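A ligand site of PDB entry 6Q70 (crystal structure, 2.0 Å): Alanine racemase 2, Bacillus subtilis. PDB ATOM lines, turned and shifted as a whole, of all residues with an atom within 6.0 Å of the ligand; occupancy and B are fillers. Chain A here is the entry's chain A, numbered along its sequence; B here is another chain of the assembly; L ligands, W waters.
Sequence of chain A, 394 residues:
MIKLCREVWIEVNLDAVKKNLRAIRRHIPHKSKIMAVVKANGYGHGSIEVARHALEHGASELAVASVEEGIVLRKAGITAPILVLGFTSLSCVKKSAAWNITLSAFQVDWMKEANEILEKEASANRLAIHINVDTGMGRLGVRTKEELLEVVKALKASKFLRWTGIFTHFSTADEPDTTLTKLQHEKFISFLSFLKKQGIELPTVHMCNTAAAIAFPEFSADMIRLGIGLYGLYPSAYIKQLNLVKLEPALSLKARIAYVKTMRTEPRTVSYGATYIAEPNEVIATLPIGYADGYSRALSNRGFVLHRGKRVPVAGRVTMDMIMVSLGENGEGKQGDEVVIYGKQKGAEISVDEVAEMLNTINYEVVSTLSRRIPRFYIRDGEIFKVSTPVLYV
OG1 of Thr 210 lies within hydrogen-bond range of O5 of the ligand (2.5 Å).
O4 of the ligand lies within hydrogen-bond range of OH of Tyr 43 (2.5 Å).
N of Ile 228 is in hydrogen-bond range of O4 of the ligand (2.9 Å).
A ring nitrogen (ND1) of His 169 lies within hydrogen-bond range of a nitrogen (N1) of the ligand.
The backbone NH (N) of Thr 210 sits at hydrogen-bond distance from an oxygen (O5) of the ligand (2.8 Å).
NE of Arg 225 lies within hydrogen-bond range of N1 of the ligand (2.8 Å).
O3 of the ligand sits at hydrogen-bond distance from OH of Tyr 364 (2.5 Å).
An oxygen (O1) of the ligand lies close to the guanidinium group of Arg 139, 3.4 Å away.
An oxygen (O5) of the ligand lies within hydrogen-bond range of the backbone NH of Gly 227 (3.1 Å).
NZ of Lys 39 is covalently linked to C5 of the ligand, 1.3 Å away.
The side-chain amide oxygen (OD1) of Asn 209 sits close to the backbone NH (N) of Ala 211.
OG1 of Thr 210 sits at hydrogen-bond distance from N of Gly 229 (3.1 Å).
The backbone NH (N) of Val 37 is in hydrogen-bond range of the backbone carbonyl oxygen (O) of Leu 226, at 2.9 Å.
A ring nitrogen (ND1) of His 169 sits at hydrogen-bond distance from the guanidinium group of Arg 225 (3.1 Å).
The side-chain hydroxyl (OG1) of Thr 210 is in hydrogen-bond range of the backbone NH (N) of Ile 228, at 3.4 Å.
The guanidinium group of Arg 225 sits at hydrogen-bond distance from the backbone carbonyl oxygen of Thr 168, 2.9 Å away.
A ring nitrogen (NE2) of His 169 is in hydrogen-bond range of the side-chain hydroxyl (OH) of Tyr 272 of chain B (2.4 Å).
OH of Tyr 43 sits at hydrogen-bond distance from NZ of Lys 39, at 3.3 Å.
Water W2 bridges O1 of the ligand (2.4 Å) and NH2 of Arg 139 (3.3 Å).
Water W4 lies within hydrogen-bond range of the side-chain hydroxyl (OH) of Tyr 272 of chain B (2.6 Å), an oxygen (O3) of the ligand (2.7 Å), the side-chain amide nitrogen (ND2) of Asn 209 (3.0 Å) and a ring nitrogen (NE2) of His 169 (3.4 Å).
Val 37 touches the ligand.
CD1 of Leu 85 touches O1 of the ligand, at 3.5 Å.
CB of Asn 209 touches O2 of the ligand (3.6 Å).
Of the 24 residues printed, 12 come within 4 Å of the ligand.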
ATOM      1  N   VAL A  37      21.878 -15.776   4.004  1.00  0.00           N
ATOM      2  CA  VAL A  37      21.357 -15.899   5.348  1.00  0.00           C
ATOM      3  C   VAL A  37      19.854 -16.193   5.421  1.00  0.00           C
ATOM      4  O   VAL A  37      18.987 -15.386   5.055  1.00  0.00           O
ATOM      5  CB  VAL A  37      21.737 -14.678   6.211  1.00  0.00           C
ATOM      6  CG1 VAL A  37      21.434 -14.982   7.665  1.00  0.00           C
ATOM      7  CG2 VAL A  37      23.208 -14.403   6.118  1.00  0.00           C
ATOM      8  N   LYS A  39      18.432 -17.937   8.191  1.00  0.00           N
ATOM      9  CA  LYS A  39      17.998 -18.234   9.594  1.00  0.00           C
ATOM     10  C   LYS A  39      16.580 -17.746   9.761  1.00  0.00           C
ATOM     11  O   LYS A  39      16.085 -16.918   8.995  1.00  0.00           O
ATOM     12  CB  LYS A  39      19.014 -17.592  10.531  1.00  0.00           C
ATOM     13  CG  LYS A  39      19.056 -16.102  10.748  1.00  0.00           C
ATOM     14  CD  LYS A  39      20.373 -15.383  11.235  1.00  0.00           C
ATOM     15  CE  LYS A  39      20.377 -13.932  12.051  1.00  0.00           C
ATOM     16  NZ  LYS A  39      20.975 -13.071  11.195  1.00  0.00           N
ATOM     17  N   TYR A  43      14.068 -15.408   7.493  1.00  0.00           N
ATOM     18  CA  TYR A  43      13.602 -14.026   7.887  1.00  0.00           C
ATOM     19  C   TYR A  43      12.085 -13.986   7.643  1.00  0.00           C
ATOM     20  O   TYR A  43      11.479 -12.902   7.164  1.00  0.00           O
ATOM     21  CB  TYR A  43      14.316 -12.889   7.121  1.00  0.00           C
ATOM     22  CG  TYR A  43      15.720 -12.578   7.526  1.00  0.00           C
ATOM     23  CD1 TYR A  43      16.632 -13.562   7.876  1.00  0.00           C
ATOM     24  CD2 TYR A  43      16.152 -11.261   7.553  1.00  0.00           C
ATOM     25  CE1 TYR A  43      17.921 -13.273   8.150  1.00  0.00           C
ATOM     26  CE2 TYR A  43      17.439 -10.966   7.814  1.00  0.00           C
ATOM     27  CZ  TYR A  43      18.363 -11.971   8.112  1.00  0.00           C
ATOM     28  OH  TYR A  43      19.692 -11.664   8.454  1.00  0.00           O
ATOM     29  N   LEU A  85      25.329 -20.227  12.623  1.00  0.00           N
ATOM     30  CA  LEU A  85      25.961 -18.994  13.185  1.00  0.00           C
ATOM     31  C   LEU A  85      25.994 -18.922  14.692  1.00  0.00           C
ATOM     32  O   LEU A  85      26.804 -18.184  15.188  1.00  0.00           O
ATOM     33  CB  LEU A  85      25.149 -17.776  12.764  1.00  0.00           C
ATOM     34  CG  LEU A  85      25.261 -17.527  11.293  1.00  0.00           C
ATOM     35  CD1 LEU A  85      24.155 -16.553  10.902  1.00  0.00           C
ATOM     36  CD2 LEU A  85      26.607 -16.977  10.758  1.00  0.00           C
ATOM     37  N   ASN A 132      34.534 -18.191  14.835  1.00  0.00           N
ATOM     38  CA  ASN A 132      33.970 -16.873  15.043  1.00  0.00           C
ATOM     39  C   ASN A 132      35.016 -16.128  15.828  1.00  0.00           C
ATOM     40  O   ASN A 132      35.365 -16.537  16.969  1.00  0.00           O
ATOM     41  CB  ASN A 132      32.664 -16.925  15.879  1.00  0.00           C
ATOM     42  CG  ASN A 132      32.004 -15.546  16.099  1.00  0.00           C
ATOM     43  OD1 ASN A 132      32.607 -14.434  15.879  1.00  0.00           O
ATOM     44  ND2 ASN A 132      30.732 -15.602  16.450  1.00  0.00           N
ATOM     45  N   ARG A 139      29.127 -10.891  21.398  1.00  0.00           N
ATOM     46  CA  ARG A 139      28.086 -11.873  21.402  1.00  0.00           C
ATOM     47  C   ARG A 139      28.671 -13.251  21.592  1.00  0.00           C
ATOM     48  O   ARG A 139      28.448 -13.875  22.642  1.00  0.00           O
ATOM     49  CB  ARG A 139      27.241 -11.804  20.104  1.00  0.00           C
ATOM     50  CG  ARG A 139      26.128 -12.861  20.049  1.00  0.00           C
ATOM     51  CD  ARG A 139      25.014 -12.485  19.023  1.00  0.00           C
ATOM     52  NE  ARG A 139      25.506 -12.436  17.654  1.00  0.00           N
ATOM     53  CZ  ARG A 139      24.845 -12.150  16.575  1.00  0.00           C
ATOM     54  NH1 ARG A 139      23.623 -11.668  16.631  1.00  0.00           N
ATOM     55  NH2 ARG A 139      25.536 -12.121  15.376  1.00  0.00           N
ATOM     56  N   PHE A 167      35.325 -16.003  10.559  1.00  0.00           N
ATOM     57  CA  PHE A 167      34.593 -14.759  10.386  1.00  0.00           C
ATOM     58  C   PHE A 167      34.533 -13.874  11.557  1.00  0.00           C
ATOM     59  O   PHE A 167      34.801 -14.305  12.651  1.00  0.00           O
ATOM     60  CB  PHE A 167      33.175 -15.105   9.918  1.00  0.00           C
ATOM     61  CG  PHE A 167      32.334 -15.865  11.003  1.00  0.00           C
ATOM     62  CD1 PHE A 167      32.400 -17.196  11.122  1.00  0.00           C
ATOM     63  CD2 PHE A 167      31.502 -15.208  11.793  1.00  0.00           C
ATOM     64  CE1 PHE A 167      31.599 -17.880  12.040  1.00  0.00           C
ATOM     65  CE2 PHE A 167      30.712 -15.851  12.762  1.00  0.00           C
ATOM     66  CZ  PHE A 167      30.782 -17.197  12.865  1.00  0.00           C
ATOM     67  N   THR A 168      34.040 -12.643  11.320  1.00  0.00           N
ATOM     68  CA  THR A 168      33.596 -11.793  12.392  1.00  0.00           C
ATOM     69  C   THR A 168      32.267 -11.142  11.966  1.00  0.00           C
ATOM     70  O   THR A 168      31.825 -11.242  10.814  1.00  0.00           O
ATOM     71  CB  THR A 168      34.638 -10.729  12.796  1.00  0.00           C
ATOM     72  OG1 THR A 168      34.242 -10.044  14.034  1.00  0.00           O
ATOM     73  CG2 THR A 168      34.786  -9.759  11.747  1.00  0.00           C
ATOM     74  N   HIS A 169      31.629 -10.468  12.921  1.00  0.00           N
ATOM     75  CA  HIS A 169      30.469  -9.770  12.678  1.00  0.00           C
ATOM     76  C   HIS A 169      30.555  -8.288  13.036  1.00  0.00           C
ATOM     77  O   HIS A 169      30.907  -7.917  14.162  1.00  0.00           O
ATOM     78  CB  HIS A 169      29.343 -10.469  13.459  1.00  0.00           C
ATOM     79  CG  HIS A 169      27.957 -10.124  12.966  1.00  0.00           C
ATOM     80  ND1 HIS A 169      27.588 -10.196  11.642  1.00  0.00           N
ATOM     81  CD2 HIS A 169      26.873  -9.627  13.624  1.00  0.00           C
ATOM     82  CE1 HIS A 169      26.350  -9.767  11.490  1.00  0.00           C
ATOM     83  NE2 HIS A 169      25.877  -9.440  12.679  1.00  0.00           N
ATOM     84  N   CYS A 208      31.338  -9.343   6.030  1.00  0.00           N
ATOM     85  CA  CYS A 208      30.281  -8.421   5.685  1.00  0.00           C
ATOM     86  C   CYS A 208      28.906  -9.027   5.814  1.00  0.00           C
ATOM     87  O   CYS A 208      28.683 -10.235   5.366  1.00  0.00           O
ATOM     88  CB  CYS A 208      30.428  -8.032   4.217  1.00  0.00           C
ATOM     89  SG  CYS A 208      31.818  -6.988   3.875  1.00  0.00           S
ATOM     90  N   ASN A 209      28.018  -8.198   6.380  1.00  0.00           N
ATOM     91  CA  ASN A 209      26.597  -8.387   6.398  1.00  0.00           C
ATOM     92  C   ASN A 209      26.146  -7.518   5.279  1.00  0.00           C
ATOM     93  O   ASN A 209      26.991  -7.023   4.555  1.00  0.00           O
ATOM     94  CB  ASN A 209      25.973  -8.003   7.740  1.00  0.00           C
ATOM     95  CG  ASN A 209      26.372  -6.554   8.220  1.00  0.00           C
ATOM     96  OD1 ASN A 209      27.041  -5.814   7.525  1.00  0.00           O
ATOM     97  ND2 ASN A 209      25.929  -6.211   9.413  1.00  0.00           N
ATOM     98  N   THR A 210      24.819  -7.374   5.068  1.00  0.00           N
ATOM     99  CA  THR A 210      24.273  -6.602   3.970  1.00  0.00           C
ATOM    100  C   THR A 210      24.852  -5.146   4.062  1.00  0.00           C
ATOM    101  O   THR A 210      25.401  -4.609   3.057  1.00  0.00           O
ATOM    102  CB  THR A 210      22.721  -6.585   4.038  1.00  0.00           C
ATOM    103  OG1 THR A 210      22.186  -7.922   3.920  1.00  0.00           O
ATOM    104  CG2 THR A 210      22.093  -5.707   3.020  1.00  0.00           C
ATOM    105  N   ALA A 211      24.760  -4.558   5.255  1.00  0.00           N
ATOM    106  CA  ALA A 211      25.189  -3.131   5.402  1.00  0.00           C
ATOM    107  C   ALA A 211      26.668  -2.961   4.967  1.00  0.00           C
ATOM    108  O   ALA A 211      26.987  -2.041   4.228  1.00  0.00           O
ATOM    109  CB  ALA A 211      24.942  -2.647   6.781  1.00  0.00           C
ATOM    110  N   ARG A 225      28.040 -12.386   3.953  1.00  0.00           N
ATOM    111  CA  ARG A 225      26.765 -12.986   4.501  1.00  0.00           C
ATOM    112  C   ARG A 225      25.603 -12.085   4.185  1.00  0.00           C
ATOM    113  O   ARG A 225      25.413 -11.036   4.867  1.00  0.00           O
ATOM    114  CB  ARG A 225      26.906 -13.318   5.958  1.00  0.00           C
ATOM    115  CG  ARG A 225      28.067 -14.282   6.290  1.00  0.00           C
ATOM    116  CD  ARG A 225      28.007 -14.624   7.754  1.00  0.00           C
ATOM    117  NE  ARG A 225      28.176 -13.378   8.508  1.00  0.00           N
ATOM    118  CZ  ARG A 225      29.345 -12.781   8.827  1.00  0.00           C
ATOM    119  NH1 ARG A 225      30.493 -13.231   8.494  1.00  0.00           N
ATOM    120  NH2 ARG A 225      29.310 -11.656   9.517  1.00  0.00           N
ATOM    121  N   LEU A 226      24.856 -12.399   3.119  1.00  0.00           N
ATOM    122  CA  LEU A 226      23.812 -11.548   2.665  1.00  0.00           C
ATOM    123  C   LEU A 226      22.500 -11.982   3.367  1.00  0.00           C
ATOM    124  O   LEU A 226      21.926 -13.042   3.011  1.00  0.00           O
ATOM    125  CB  LEU A 226      23.618 -11.690   1.162  1.00  0.00           C
ATOM    126  CG  LEU A 226      22.561 -10.741   0.600  1.00  0.00           C
ATOM    127  CD1 LEU A 226      22.909  -9.259   0.888  1.00  0.00           C
ATOM    128  CD2 LEU A 226      22.399 -11.048  -0.872  1.00  0.00           C
ATOM    129  N   GLY A 227      22.018 -11.153   4.306  1.00  0.00           N
ATOM    130  CA  GLY A 227      20.726 -11.450   4.953  1.00  0.00           C
ATOM    131  C   GLY A 227      19.602 -10.574   4.444  1.00  0.00           C
ATOM    132  O   GLY A 227      18.851 -10.885   3.444  1.00  0.00           O
ATOM    133  N   ILE A 228      19.431  -9.441   5.133  1.00  0.00           N
ATOM    134  CA  ILE A 228      18.290  -8.588   4.909  1.00  0.00           C
ATOM    135  C   ILE A 228      18.168  -8.142   3.443  1.00  0.00           C
ATOM    136  O   ILE A 228      17.025  -8.076   2.856  1.00  0.00           O
ATOM    137  CB  ILE A 228      18.250  -7.413   5.936  1.00  0.00           C
ATOM    138  CG1 ILE A 228      16.906  -6.700   5.966  1.00  0.00           C
ATOM    139  CG2 ILE A 228      19.315  -6.369   5.545  1.00  0.00           C
ATOM    140  CD1 ILE A 228      15.693  -7.489   6.426  1.00  0.00           C
ATOM    141  N   GLY A 229      19.304  -7.780   2.867  1.00  0.00           N
ATOM    142  CA  GLY A 229      19.378  -7.493   1.421  1.00  0.00           C
ATOM    143  C   GLY A 229      18.811  -8.555   0.465  1.00  0.00           C
ATOM    144  O   GLY A 229      17.992  -8.279  -0.573  1.00  0.00           O
ATOM    145  N   PRO A 235      19.270  -2.468   5.518  1.00  0.00           N
ATOM    146  CA  PRO A 235      19.534  -2.640   6.934  1.00  0.00           C
ATOM    147  C   PRO A 235      19.228  -1.402   7.766  1.00  0.00           C
ATOM    148  O   PRO A 235      19.027  -1.546   8.975  1.00  0.00           O
ATOM    149  CB  PRO A 235      21.063  -2.868   7.009  1.00  0.00           C
ATOM    150  CG  PRO A 235      21.537  -2.804   5.659  1.00  0.00           C
ATOM    151  CD  PRO A 235      20.443  -2.662   4.696  1.00  0.00           C
ATOM    152  N   TYR A 364      13.656  -6.212   9.988  1.00  0.00           N
ATOM    153  CA  TYR A 364      14.018  -7.566  10.421  1.00  0.00           C
ATOM    154  C   TYR A 364      13.040  -8.207  11.346  1.00  0.00           C
ATOM    155  O   TYR A 364      12.698  -9.400  11.129  1.00  0.00           O
ATOM    156  CB  TYR A 364      15.360  -7.570  11.195  1.00  0.00           C
ATOM    157  CG  TYR A 364      16.638  -7.083  10.485  1.00  0.00           C
ATOM    158  CD1 TYR A 364      16.999  -5.735  10.466  1.00  0.00           C
ATOM    159  CD2 TYR A 364      17.565  -7.991  10.002  1.00  0.00           C
ATOM    160  CE1 TYR A 364      18.198  -5.300   9.861  1.00  0.00           C
ATOM    161  CE2 TYR A 364      18.773  -7.587   9.460  1.00  0.00           C
ATOM    162  CZ  TYR A 364      19.068  -6.237   9.387  1.00  0.00           C
ATOM    163  OH  TYR A 364      20.239  -5.882   8.770  1.00  0.00           O
ATOM    164  N   TYR B 272      24.216  -5.105  18.650  1.00  0.00           N
ATOM    165  CA  TYR B 272      23.982  -4.165  17.560  1.00  0.00           C
ATOM    166  C   TYR B 272      23.790  -2.770  18.128  1.00  0.00           C
ATOM    167  O   TYR B 272      23.252  -2.583  19.184  1.00  0.00           O
ATOM    168  CB  TYR B 272      22.788  -4.564  16.770  1.00  0.00           C
ATOM    169  CG  TYR B 272      22.997  -5.699  15.843  1.00  0.00           C
ATOM    170  CD1 TYR B 272      23.902  -5.568  14.816  1.00  0.00           C
ATOM    171  CD2 TYR B 272      22.187  -6.852  15.905  1.00  0.00           C
ATOM    172  CE1 TYR B 272      24.074  -6.586  13.889  1.00  0.00           C
ATOM    173  CE2 TYR B 272      22.358  -7.918  14.986  1.00  0.00           C
ATOM    174  CZ  TYR B 272      23.310  -7.745  13.973  1.00  0.00           C
ATOM    175  OH  TYR B 272      23.578  -8.717  13.087  1.00  0.00           O
ATOM    176  N   MET B 320      18.357 -11.295  16.405  1.00  0.00           N
ATOM    177  CA  MET B 320      17.337 -12.096  15.796  1.00  0.00           C
ATOM    178  C   MET B 320      17.251 -13.438  16.513  1.00  0.00           C
ATOM    179  O   MET B 320      16.166 -13.917  16.737  1.00  0.00           O
ATOM    180  CB  MET B 320      17.587 -12.265  14.296  1.00  0.00           C
ATOM    181  CG  MET B 320      16.450 -13.089  13.675  1.00  0.00           C
ATOM    182  SD  MET B 320      16.544 -13.197  11.909  1.00  0.00           S
ATOM    183  CE  MET B 320      16.143 -11.503  11.477  1.00  0.00           C
ATOM    184  N   ASP B 321      18.398 -13.995  16.933  1.00  0.00           N
ATOM    185  CA  ASP B 321      18.477 -15.330  17.519  1.00  0.00           C
ATOM    186  C   ASP B 321      19.099 -15.409  18.899  1.00  0.00           C
ATOM    187  O   ASP B 321      19.063 -16.484  19.489  1.00  0.00           O
ATOM    188  CB  ASP B 321      19.229 -16.288  16.565  1.00  0.00           C
ATOM    189  CG  ASP B 321      18.743 -16.188  15.128  1.00  0.00           C
ATOM    190  OD1 ASP B 321      17.470 -16.295  14.935  1.00  0.00           O
ATOM    191  OD2 ASP B 321      19.626 -15.938  14.276  1.00  0.00           O
ATOM    192  N   MET B 322      19.615 -14.303  19.454  1.00  0.00           N
ATOM    193  CA  MET B 322      20.360 -14.317  20.690  1.00  0.00           C
ATOM    194  C   MET B 322      20.211 -12.984  21.445  1.00  0.00           C
ATOM    195  O   MET B 322      19.856 -11.918  20.842  1.00  0.00           O
ATOM    196  CB  MET B 322      21.847 -14.557  20.431  1.00  0.00           C
ATOM    197  CG  MET B 322      22.361 -16.001  20.175  1.00  0.00           C
ATOM    198  SD  MET B 322      24.102 -16.066  19.530  1.00  0.00           S
ATOM    199  CE  MET B 322      23.945 -15.883  17.762  1.00  0.00           C
HETATM  200  N1  LIG L   1      26.330 -12.354  10.368  1.00  0.00           N
HETATM  201  C1  LIG L   1      25.912 -12.899  11.517  1.00  0.00           C
HETATM  202  C2  LIG L   1      26.986 -13.319  12.575  1.00  0.00           C
HETATM  203  C3  LIG L   1      24.381 -13.029  11.628  1.00  0.00           C
HETATM  204  O1  LIG L   1      23.941 -13.612  12.745  1.00  0.00           O
HETATM  205  C4  LIG L   1      23.471 -12.540  10.543  1.00  0.00           C
HETATM  206  C5  LIG L   1      21.985 -12.699  10.425  1.00  0.00           C
HETATM  207  C6  LIG L   1      24.192 -11.908   9.339  1.00  0.00           C
HETATM  208  C7  LIG L   1      25.577 -11.856   9.361  1.00  0.00           C
HETATM  209  C8  LIG L   1      23.555 -11.201   8.101  1.00  0.00           C
HETATM  210  O2  LIG L   1      22.992  -9.891   8.576  1.00  0.00           O
HETATM  211  P1  LIG L   1      22.058  -8.874   7.655  1.00  0.00           P
HETATM  212  O3  LIG L   1      22.043  -7.535   8.522  1.00  0.00           O
HETATM  213  O4  LIG L   1      20.793  -9.615   7.661  1.00  0.00           O
HETATM  214  O5  LIG L   1      22.669  -8.839   6.191  1.00  0.00           O
HETATM  215  O   HOH W   1      26.779 -15.394  15.326  1.00  0.00           O
HETATM  216  O   HOH W   2      23.897 -14.938  14.781  1.00  0.00           O
HETATM  217  O   HOH W   3      23.346  -5.515   7.574  1.00  0.00           O
HETATM  218  O   HOH W   4      23.697  -7.735  10.701  1.00  0.00           O
